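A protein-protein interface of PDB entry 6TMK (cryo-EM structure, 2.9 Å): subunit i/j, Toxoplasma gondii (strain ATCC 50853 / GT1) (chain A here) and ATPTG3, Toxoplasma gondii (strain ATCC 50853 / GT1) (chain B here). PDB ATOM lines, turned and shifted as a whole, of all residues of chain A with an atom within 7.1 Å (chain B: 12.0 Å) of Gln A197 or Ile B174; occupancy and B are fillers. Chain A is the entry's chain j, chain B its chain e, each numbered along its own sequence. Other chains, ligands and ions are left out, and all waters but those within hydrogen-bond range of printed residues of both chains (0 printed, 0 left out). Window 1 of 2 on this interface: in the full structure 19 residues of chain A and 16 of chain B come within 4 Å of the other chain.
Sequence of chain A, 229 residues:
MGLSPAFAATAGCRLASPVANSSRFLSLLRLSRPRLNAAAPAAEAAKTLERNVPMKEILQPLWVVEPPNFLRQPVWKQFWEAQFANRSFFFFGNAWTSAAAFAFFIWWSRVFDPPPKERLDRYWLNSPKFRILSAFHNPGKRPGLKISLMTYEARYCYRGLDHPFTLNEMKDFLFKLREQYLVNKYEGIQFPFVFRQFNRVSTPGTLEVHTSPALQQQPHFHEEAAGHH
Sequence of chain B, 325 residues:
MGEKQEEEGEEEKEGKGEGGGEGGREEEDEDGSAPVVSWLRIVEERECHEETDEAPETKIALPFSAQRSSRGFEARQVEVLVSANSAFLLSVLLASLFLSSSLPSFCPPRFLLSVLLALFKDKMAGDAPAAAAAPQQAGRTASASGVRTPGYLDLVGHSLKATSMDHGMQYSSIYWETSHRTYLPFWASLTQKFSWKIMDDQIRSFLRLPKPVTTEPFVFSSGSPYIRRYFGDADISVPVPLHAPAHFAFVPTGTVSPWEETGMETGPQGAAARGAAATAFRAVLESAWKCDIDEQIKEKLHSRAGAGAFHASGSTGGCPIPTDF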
ATOM      1  N   ARG A 142     -26.279  27.720  -3.377  1.00  0.00           N
ATOM      2  CA  ARG A 142     -26.296  26.728  -4.449  1.00  0.00           C
ATOM      3  C   ARG A 142     -27.682  26.103  -4.496  1.00  0.00           C
ATOM      4  O   ARG A 142     -27.997  25.229  -3.670  1.00  0.00           O
ATOM      5  CB  ARG A 142     -25.230  25.669  -4.236  1.00  0.00           C
ATOM      6  CG  ARG A 142     -23.825  26.172  -4.398  1.00  0.00           C
ATOM      7  CD  ARG A 142     -22.819  25.091  -4.143  1.00  0.00           C
ATOM      8  NE  ARG A 142     -22.878  24.026  -5.133  1.00  0.00           N
ATOM      9  CZ  ARG A 142     -22.320  24.082  -6.333  1.00  0.00           C
ATOM     10  NH1 ARG A 142     -22.431  23.060  -7.155  1.00  0.00           N
ATOM     11  NH2 ARG A 142     -21.655  25.152  -6.715  1.00  0.00           N
ATOM     12  N   ILE A 189     -13.657  25.127  -0.815  1.00  0.00           N
ATOM     13  CA  ILE A 189     -13.535  23.965  -1.678  1.00  0.00           C
ATOM     14  C   ILE A 189     -14.068  24.287  -3.071  1.00  0.00           C
ATOM     15  O   ILE A 189     -14.970  25.113  -3.247  1.00  0.00           O
ATOM     16  CB  ILE A 189     -14.268  22.776  -1.033  1.00  0.00           C
ATOM     17  CG1 ILE A 189     -13.922  21.464  -1.727  1.00  0.00           C
ATOM     18  CG2 ILE A 189     -15.760  23.016  -0.995  1.00  0.00           C
ATOM     19  CD1 ILE A 189     -14.379  20.283  -0.972  1.00  0.00           C
ATOM     20  N   GLN A 190     -13.502  23.620  -4.069  1.00  0.00           N
ATOM     21  CA  GLN A 190     -13.631  24.060  -5.450  1.00  0.00           C
ATOM     22  C   GLN A 190     -13.707  22.810  -6.328  1.00  0.00           C
ATOM     23  O   GLN A 190     -13.895  21.696  -5.832  1.00  0.00           O
ATOM     24  CB  GLN A 190     -12.484  25.039  -5.732  1.00  0.00           C
ATOM     25  CG  GLN A 190     -12.811  26.081  -6.728  1.00  0.00           C
ATOM     26  CD  GLN A 190     -12.057  27.348  -6.484  1.00  0.00           C
ATOM     27  OE1 GLN A 190     -11.547  27.594  -5.396  1.00  0.00           O
ATOM     28  NE2 GLN A 190     -12.034  28.191  -7.473  1.00  0.00           N
ATOM     29  N   PHE A 191     -13.517  22.966  -7.645  1.00  0.00           N
ATOM     30  CA  PHE A 191     -14.053  22.056  -8.658  1.00  0.00           C
ATOM     31  C   PHE A 191     -13.808  20.577  -8.411  1.00  0.00           C
ATOM     32  O   PHE A 191     -14.775  19.810  -8.319  1.00  0.00           O
ATOM     33  CB  PHE A 191     -13.577  22.355 -10.075  1.00  0.00           C
ATOM     34  CG  PHE A 191     -13.672  21.159 -10.971  1.00  0.00           C
ATOM     35  CD1 PHE A 191     -14.878  20.551 -11.210  1.00  0.00           C
ATOM     36  CD2 PHE A 191     -12.550  20.660 -11.596  1.00  0.00           C
ATOM     37  CE1 PHE A 191     -14.955  19.435 -11.998  1.00  0.00           C
ATOM     38  CE2 PHE A 191     -12.632  19.551 -12.395  1.00  0.00           C
ATOM     39  CZ  PHE A 191     -13.838  18.954 -12.610  1.00  0.00           C
ATOM     40  N   PRO A 192     -12.563  20.124  -8.303  1.00  0.00           N
ATOM     41  CA  PRO A 192     -12.304  18.683  -8.404  1.00  0.00           C
ATOM     42  C   PRO A 192     -13.062  17.888  -7.368  1.00  0.00           C
ATOM     43  O   PRO A 192     -13.322  16.701  -7.587  1.00  0.00           O
ATOM     44  CB  PRO A 192     -10.782  18.581  -8.223  1.00  0.00           C
ATOM     45  CG  PRO A 192     -10.276  19.933  -8.468  1.00  0.00           C
ATOM     46  CD  PRO A 192     -11.334  20.888  -8.067  1.00  0.00           C
ATOM     47  N   VAL A 194     -16.010  19.441  -5.646  1.00  0.00           N
ATOM     48  CA  VAL A 194     -17.392  19.878  -5.810  1.00  0.00           C
ATOM     49  C   VAL A 194     -17.464  20.744  -7.053  1.00  0.00           C
ATOM     50  O   VAL A 194     -16.528  21.479  -7.369  1.00  0.00           O
ATOM     51  CB  VAL A 194     -17.917  20.684  -4.602  1.00  0.00           C
ATOM     52  CG1 VAL A 194     -17.759  19.931  -3.326  1.00  0.00           C
ATOM     53  CG2 VAL A 194     -17.187  22.003  -4.513  1.00  0.00           C
ATOM     54  N   PHE A 195     -18.587  20.665  -7.761  1.00  0.00           N
ATOM     55  CA  PHE A 195     -18.749  21.429  -8.996  1.00  0.00           C
ATOM     56  C   PHE A 195     -18.916  22.896  -8.638  1.00  0.00           C
ATOM     57  O   PHE A 195     -20.016  23.358  -8.335  1.00  0.00           O
ATOM     58  CB  PHE A 195     -19.940  20.929  -9.800  1.00  0.00           C
ATOM     59  CG  PHE A 195     -19.665  19.688 -10.581  1.00  0.00           C
ATOM     60  CD1 PHE A 195     -18.741  19.681 -11.601  1.00  0.00           C
ATOM     61  CD2 PHE A 195     -20.344  18.526 -10.305  1.00  0.00           C
ATOM     62  CE1 PHE A 195     -18.494  18.541 -12.306  1.00  0.00           C
ATOM     63  CE2 PHE A 195     -20.100  17.393 -11.009  1.00  0.00           C
ATOM     64  CZ  PHE A 195     -19.176  17.400 -12.015  1.00  0.00           C
ATOM     65  N   ARG A 196     -17.819  23.639  -8.693  1.00  0.00           N
ATOM     66  CA  ARG A 196     -17.808  25.027  -8.271  1.00  0.00           C
ATOM     67  C   ARG A 196     -16.485  25.638  -8.690  1.00  0.00           C
ATOM     68  O   ARG A 196     -15.437  25.009  -8.550  1.00  0.00           O
ATOM     69  CB  ARG A 196     -18.004  25.137  -6.756  1.00  0.00           C
ATOM     70  CG  ARG A 196     -17.886  26.524  -6.203  1.00  0.00           C
ATOM     71  CD  ARG A 196     -18.563  26.687  -4.876  1.00  0.00           C
ATOM     72  NE  ARG A 196     -17.671  26.479  -3.749  1.00  0.00           N
ATOM     73  CZ  ARG A 196     -17.900  26.943  -2.529  1.00  0.00           C
ATOM     74  NH1 ARG A 196     -18.992  27.637  -2.275  1.00  0.00           N
ATOM     75  NH2 ARG A 196     -17.036  26.703  -1.563  1.00  0.00           N
ATOM     76  N   GLN A 197     -16.550  26.850  -9.226  1.00  0.00           N
ATOM     77  CA  GLN A 197     -15.371  27.583  -9.655  1.00  0.00           C
ATOM     78  C   GLN A 197     -15.522  29.045  -9.278  1.00  0.00           C
ATOM     79  O   GLN A 197     -16.547  29.661  -9.577  1.00  0.00           O
ATOM     80  CB  GLN A 197     -15.147  27.449 -11.162  1.00  0.00           C
ATOM     81  CG  GLN A 197     -14.948  26.045 -11.654  1.00  0.00           C
ATOM     82  CD  GLN A 197     -16.139  25.489 -12.388  1.00  0.00           C
ATOM     83  OE1 GLN A 197     -16.933  26.223 -12.969  1.00  0.00           O
ATOM     84  NE2 GLN A 197     -16.274  24.176 -12.358  1.00  0.00           N
ATOM     85  N   PHE A 198     -14.512  29.591  -8.611  1.00  0.00           N
ATOM     86  CA  PHE A 198     -14.428  31.017  -8.360  1.00  0.00           C
ATOM     87  C   PHE A 198     -12.974  31.458  -8.433  1.00  0.00           C
ATOM     88  O   PHE A 198     -12.048  30.670  -8.235  1.00  0.00           O
ATOM     89  CB  PHE A 198     -15.081  31.413  -7.023  1.00  0.00           C
ATOM     90  CG  PHE A 198     -14.564  30.677  -5.840  1.00  0.00           C
ATOM     91  CD1 PHE A 198     -13.514  31.176  -5.110  1.00  0.00           C
ATOM     92  CD2 PHE A 198     -15.153  29.504  -5.434  1.00  0.00           C
ATOM     93  CE1 PHE A 198     -13.051  30.513  -4.022  1.00  0.00           C
ATOM     94  CE2 PHE A 198     -14.689  28.839  -4.345  1.00  0.00           C
ATOM     95  CZ  PHE A 198     -13.641  29.340  -3.636  1.00  0.00           C
ATOM     96  N   ASN A 199     -12.788  32.745  -8.713  1.00  0.00           N
ATOM     97  CA  ASN A 199     -11.499  33.314  -9.081  1.00  0.00           C
ATOM     98  C   ASN A 199     -10.724  33.839  -7.879  1.00  0.00           C
ATOM     99  O   ASN A 199      -9.521  33.595  -7.765  1.00  0.00           O
ATOM    100  CB  ASN A 199     -11.703  34.426 -10.110  1.00  0.00           C
ATOM    101  CG  ASN A 199     -10.412  34.920 -10.701  1.00  0.00           C
ATOM    102  OD1 ASN A 199     -10.030  36.067 -10.497  1.00  0.00           O
ATOM    103  ND2 ASN A 199      -9.723  34.058 -11.422  1.00  0.00           N
ATOM    104  N   HIS B 167      -9.603  25.601   0.700  1.00  0.00           N
ATOM    105  CA  HIS B 167      -8.935  26.735   0.070  1.00  0.00           C
ATOM    106  C   HIS B 167      -8.176  26.294  -1.179  1.00  0.00           C
ATOM    107  O   HIS B 167      -6.966  26.478  -1.315  1.00  0.00           O
ATOM    108  CB  HIS B 167      -8.018  27.450   1.063  1.00  0.00           C
ATOM    109  CG  HIS B 167      -8.758  28.167   2.144  1.00  0.00           C
ATOM    110  ND1 HIS B 167      -9.527  29.284   1.901  1.00  0.00           N
ATOM    111  CD2 HIS B 167      -8.851  27.926   3.472  1.00  0.00           C
ATOM    112  CE1 HIS B 167     -10.063  29.700   3.033  1.00  0.00           C
ATOM    113  NE2 HIS B 167      -9.668  28.894   4.002  1.00  0.00           N
ATOM    114  N   GLY B 168      -8.922  25.723  -2.104  1.00  0.00           N
ATOM    115  CA  GLY B 168      -8.334  25.219  -3.318  1.00  0.00           C
ATOM    116  C   GLY B 168      -8.223  26.275  -4.387  1.00  0.00           C
ATOM    117  O   GLY B 168      -8.855  27.326  -4.332  1.00  0.00           O
ATOM    118  N   MET B 169      -7.402  25.973  -5.379  1.00  0.00           N
ATOM    119  CA  MET B 169      -7.174  26.881  -6.488  1.00  0.00           C
ATOM    120  C   MET B 169      -8.194  26.658  -7.590  1.00  0.00           C
ATOM    121  O   MET B 169      -8.872  25.634  -7.656  1.00  0.00           O
ATOM    122  CB  MET B 169      -5.772  26.705  -7.068  1.00  0.00           C
ATOM    123  CG  MET B 169      -4.648  27.220  -6.193  1.00  0.00           C
ATOM    124  SD  MET B 169      -3.143  27.557  -7.121  1.00  0.00           S
ATOM    125  CE  MET B 169      -2.814  25.944  -7.818  1.00  0.00           C
ATOM    126  N   GLN B 170      -8.302  27.653  -8.455  1.00  0.00           N
ATOM    127  CA  GLN B 170      -9.184  27.552  -9.599  1.00  0.00           C
ATOM    128  C   GLN B 170      -8.596  26.530 -10.563  1.00  0.00           C
ATOM    129  O   GLN B 170      -7.501  26.719 -11.100  1.00  0.00           O
ATOM    130  CB  GLN B 170      -9.349  28.908 -10.255  1.00  0.00           C
ATOM    131  CG  GLN B 170     -10.651  29.085 -10.976  1.00  0.00           C
ATOM    132  CD  GLN B 170     -10.642  30.289 -11.879  1.00  0.00           C
ATOM    133  OE1 GLN B 170     -10.262  31.382 -11.474  1.00  0.00           O
ATOM    134  NE2 GLN B 170     -11.032  30.087 -13.122  1.00  0.00           N
ATOM    135  N   TYR B 171      -9.333  25.450 -10.774  1.00  0.00           N
ATOM    136  CA  TYR B 171      -8.883  24.288 -11.523  1.00  0.00           C
ATOM    137  C   TYR B 171      -9.383  24.289 -12.954  1.00  0.00           C
ATOM    138  O   TYR B 171      -8.686  23.801 -13.846  1.00  0.00           O
ATOM    139  CB  TYR B 171      -9.340  23.022 -10.796  1.00  0.00           C
ATOM    140  CG  TYR B 171      -8.515  21.793 -11.030  1.00  0.00           C
ATOM    141  CD1 TYR B 171      -8.988  20.758 -11.814  1.00  0.00           C
ATOM    142  CD2 TYR B 171      -7.270  21.661 -10.446  1.00  0.00           C
ATOM    143  CE1 TYR B 171      -8.243  19.622 -12.018  1.00  0.00           C
ATOM    144  CE2 TYR B 171      -6.512  20.525 -10.644  1.00  0.00           C
ATOM    145  CZ  TYR B 171      -7.003  19.512 -11.436  1.00  0.00           C
ATOM    146  OH  TYR B 171      -6.250  18.379 -11.634  1.00  0.00           O
ATOM    147  N   SER B 172     -10.575  24.819 -13.179  1.00  0.00           N
ATOM    148  CA  SER B 172     -11.181  24.936 -14.492  1.00  0.00           C
ATOM    149  C   SER B 172     -11.410  26.411 -14.784  1.00  0.00           C
ATOM    150  O   SER B 172     -11.493  27.241 -13.876  1.00  0.00           O
ATOM    151  CB  SER B 172     -12.499  24.155 -14.575  1.00  0.00           C
ATOM    152  OG  SER B 172     -12.280  22.764 -14.491  1.00  0.00           O
ATOM    153  N   SER B 173     -11.511  26.731 -16.065  1.00  0.00           N
ATOM    154  CA  SER B 173     -11.701  28.106 -16.480  1.00  0.00           C
ATOM    155  C   SER B 173     -13.172  28.502 -16.408  1.00  0.00           C
ATOM    156  O   SER B 173     -14.078  27.669 -16.475  1.00  0.00           O
ATOM    157  CB  SER B 173     -11.158  28.310 -17.893  1.00  0.00           C
ATOM    158  OG  SER B 173      -9.878  27.739 -18.034  1.00  0.00           O
ATOM    159  N   ILE B 174     -13.395  29.803 -16.272  1.00  0.00           N
ATOM    160  CA  ILE B 174     -14.726  30.390 -16.248  1.00  0.00           C
ATOM    161  C   ILE B 174     -14.862  31.272 -17.475  1.00  0.00           C
ATOM    162  O   ILE B 174     -13.965  32.066 -17.778  1.00  0.00           O
ATOM    163  CB  ILE B 174     -14.958  31.211 -14.966  1.00  0.00           C
ATOM    164  CG1 ILE B 174     -15.028  30.305 -13.746  1.00  0.00           C
ATOM    165  CG2 ILE B 174     -16.249  31.985 -15.056  1.00  0.00           C
ATOM    166  CD1 ILE B 174     -14.544  30.965 -12.505  1.00  0.00           C
ATOM    167  N   TYR B 175     -15.978  31.135 -18.178  1.00  0.00           N
ATOM    168  CA  TYR B 175     -16.151  31.841 -19.436  1.00  0.00           C
ATOM    169  C   TYR B 175     -17.626  31.919 -19.785  1.00  0.00           C
ATOM    170  O   TYR B 175     -18.469  31.226 -19.214  1.00  0.00           O
ATOM    171  CB  TYR B 175     -15.358  31.171 -20.561  1.00  0.00           C
ATOM    172  CG  TYR B 175     -15.692  29.724 -20.798  1.00  0.00           C
ATOM    173  CD1 TYR B 175     -16.725  29.361 -21.635  1.00  0.00           C
ATOM    174  CD2 TYR B 175     -14.968  28.720 -20.190  1.00  0.00           C
ATOM    175  CE1 TYR B 175     -17.028  28.051 -21.852  1.00  0.00           C
ATOM    176  CE2 TYR B 175     -15.264  27.410 -20.403  1.00  0.00           C
ATOM    177  CZ  TYR B 175     -16.295  27.075 -21.235  1.00  0.00           C
ATOM    178  OH  TYR B 175     -16.591  25.757 -21.448  1.00  0.00           O
ATOM    179  N   TRP B 176     -17.917  32.793 -20.740  1.00  0.00           N
ATOM    180  CA  TRP B 176     -19.250  32.971 -21.292  1.00  0.00           C
ATOM    181  C   TRP B 176     -19.143  32.838 -22.797  1.00  0.00           C
ATOM    182  O   TRP B 176     -18.385  33.571 -23.435  1.00  0.00           O
ATOM    183  CB  TRP B 176     -19.830  34.333 -20.919  1.00  0.00           C
ATOM    184  CG  TRP B 176     -21.305  34.423 -21.068  1.00  0.00           C
ATOM    185  CD1 TRP B 176     -21.991  34.993 -22.091  1.00  0.00           C
ATOM    186  CD2 TRP B 176     -22.282  33.928 -20.158  1.00  0.00           C
ATOM    187  NE1 TRP B 176     -23.333  34.885 -21.877  1.00  0.00           N
ATOM    188  CE2 TRP B 176     -23.540  34.231 -20.694  1.00  0.00           C
ATOM    189  CE3 TRP B 176     -22.217  33.253 -18.944  1.00  0.00           C
ATOM    190  CZ2 TRP B 176     -24.717  33.889 -20.057  1.00  0.00           C
ATOM    191  CZ3 TRP B 176     -23.378  32.915 -18.318  1.00  0.00           C
ATOM    192  CH2 TRP B 176     -24.614  33.229 -18.871  1.00  0.00           C
ATOM    193  N   GLU B 177     -19.885  31.894 -23.358  1.00  0.00           N
ATOM    194  CA  GLU B 177     -19.852  31.694 -24.793  1.00  0.00           C
ATOM    195  C   GLU B 177     -20.536  32.845 -25.509  1.00  0.00           C
ATOM    196  O   GLU B 177     -21.404  33.528 -24.961  1.00  0.00           O
ATOM    197  CB  GLU B 177     -20.509  30.369 -25.165  1.00  0.00           C
ATOM    198  CG  GLU B 177     -19.683  29.166 -24.787  1.00  0.00           C
ATOM    199  CD  GLU B 177     -20.275  27.859 -25.267  1.00  0.00           C
ATOM    200  OE1 GLU B 177     -20.941  27.851 -26.323  1.00  0.00           O
ATOM    201  OE2 GLU B 177     -20.063  26.832 -24.591  1.00  0.00           O
ATOM    202  N   THR B 178     -20.134  33.048 -26.754  1.00  0.00           N
ATOM    203  CA  THR B 178     -20.582  34.199 -27.515  1.00  0.00           C
ATOM    204  C   THR B 178     -22.090  34.139 -27.709  1.00  0.00           C
ATOM    205  O   THR B 178     -22.639  33.120 -28.136  1.00  0.00           O
ATOM    206  CB  THR B 178     -19.858  34.241 -28.857  1.00  0.00           C
ATOM    207  OG1 THR B 178     -18.449  34.152 -28.636  1.00  0.00           O
ATOM    208  CG2 THR B 178     -20.148  35.527 -29.586  1.00  0.00           C
ATOM    209  N   HIS B 180     -24.583  33.946 -25.757  1.00  0.00           N
ATOM    210  CA  HIS B 180     -25.467  33.270 -24.823  1.00  0.00           C
ATOM    211  C   HIS B 180     -26.192  34.295 -23.967  1.00  0.00           C
ATOM    212  O   HIS B 180     -25.608  35.286 -23.523  1.00  0.00           O
ATOM    213  CB  HIS B 180     -24.688  32.313 -23.929  1.00  0.00           C
ATOM    214  CG  HIS B 180     -24.396  30.990 -24.555  1.00  0.00           C
ATOM    215  ND1 HIS B 180     -23.844  29.946 -23.847  1.00  0.00           N
ATOM    216  CD2 HIS B 180     -24.572  30.537 -25.817  1.00  0.00           C
ATOM    217  CE1 HIS B 180     -23.696  28.906 -24.645  1.00  0.00           C
ATOM    218  NE2 HIS B 180     -24.128  29.239 -25.847  1.00  0.00           N
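The backbone carbonyl oxygen (O) of Gly B168 lies close to the side-chain amide oxygen (OE1) of Gln A190, at 2.9 Å. The side-chain amide oxygen (OE1) of Gln B170 sits at hydrogen-bond distance from the side-chain amide nitrogen (ND2) of Asn A199, at 2.7 Å.
NE2 of Gln A190 lies within hydrogen-bond range of O of Phe A198 (2.6 Å). The side-chain amide nitrogen (NE2) of Gln B170 sits at hydrogen-bond distance from the backbone carbonyl oxygen (O) of Ser B172, 3.0 Å away. The backbone carbonyl oxygen (O) of Arg A196 sits at hydrogen-bond distance from the backbone NH (N) of Phe A191 (2.9 Å).
Among the printed residues, merely in contact across the chains: Gln A190 with Met B169, Gln A190 with Gln B170, Phe A191 with Tyr B171, Phe A191 with Ser B172, Pro A192 with Tyr B171, Gln A197 with Ile B174 and Phe A198 with Gln B170.
Of the printed residues of chain B, Phe A191 touches Tyr B171 and Ser B172. Of the printed residues of chain B, Pro A192 touches Tyr B171. No residue of chain B comes within 4 Å of Phe A195. No residue of chain B comes within 4 Å of Arg A196. Of chain B, only Ile B174 comes within 4 Å of Gln A197. Of chain B, only Gln B170 (3.5 Å) comes within 4 Å of Phe A198. Asn A199 touches one residue of chain B. Of the printed residues of chain A, Gly B168 touches Gln A190. Of the printed residues of chain A, Met B169 touches Gln A190 (3.8 Å). Printed residues of chain A within 4 Å of Tyr B171: Phe A191 (3.6 Å) and Pro A192 (3.6 Å). Of the printed residues of chain A, Ser B172 touches Phe A191 (3.6 Å). Ile B174 touches one residue of chain A. Tyr B175 touches none of the printed residues of chain A. Trp B176 touches none of the printed residues of chain A.
Printed residues of chain B that touch a printed residue of chain A: Gly B168, Met B169, Gln B170, Tyr B171, Ser B172 and Ile B174. Of the 11 printed residues of chain A, 6 touch a printed residue of chain B. Hydrophobic or aromatic side chains of chain A within 4 Å of the printed part of chain B: Phe A191 and Pro A192. Among the printed residues, 9 pairs touch across the chains. Among the printed residues, no Asp or Glu carboxylate lies within 4 Å of a Lys or Arg side-chain nitrogen of the other chain.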
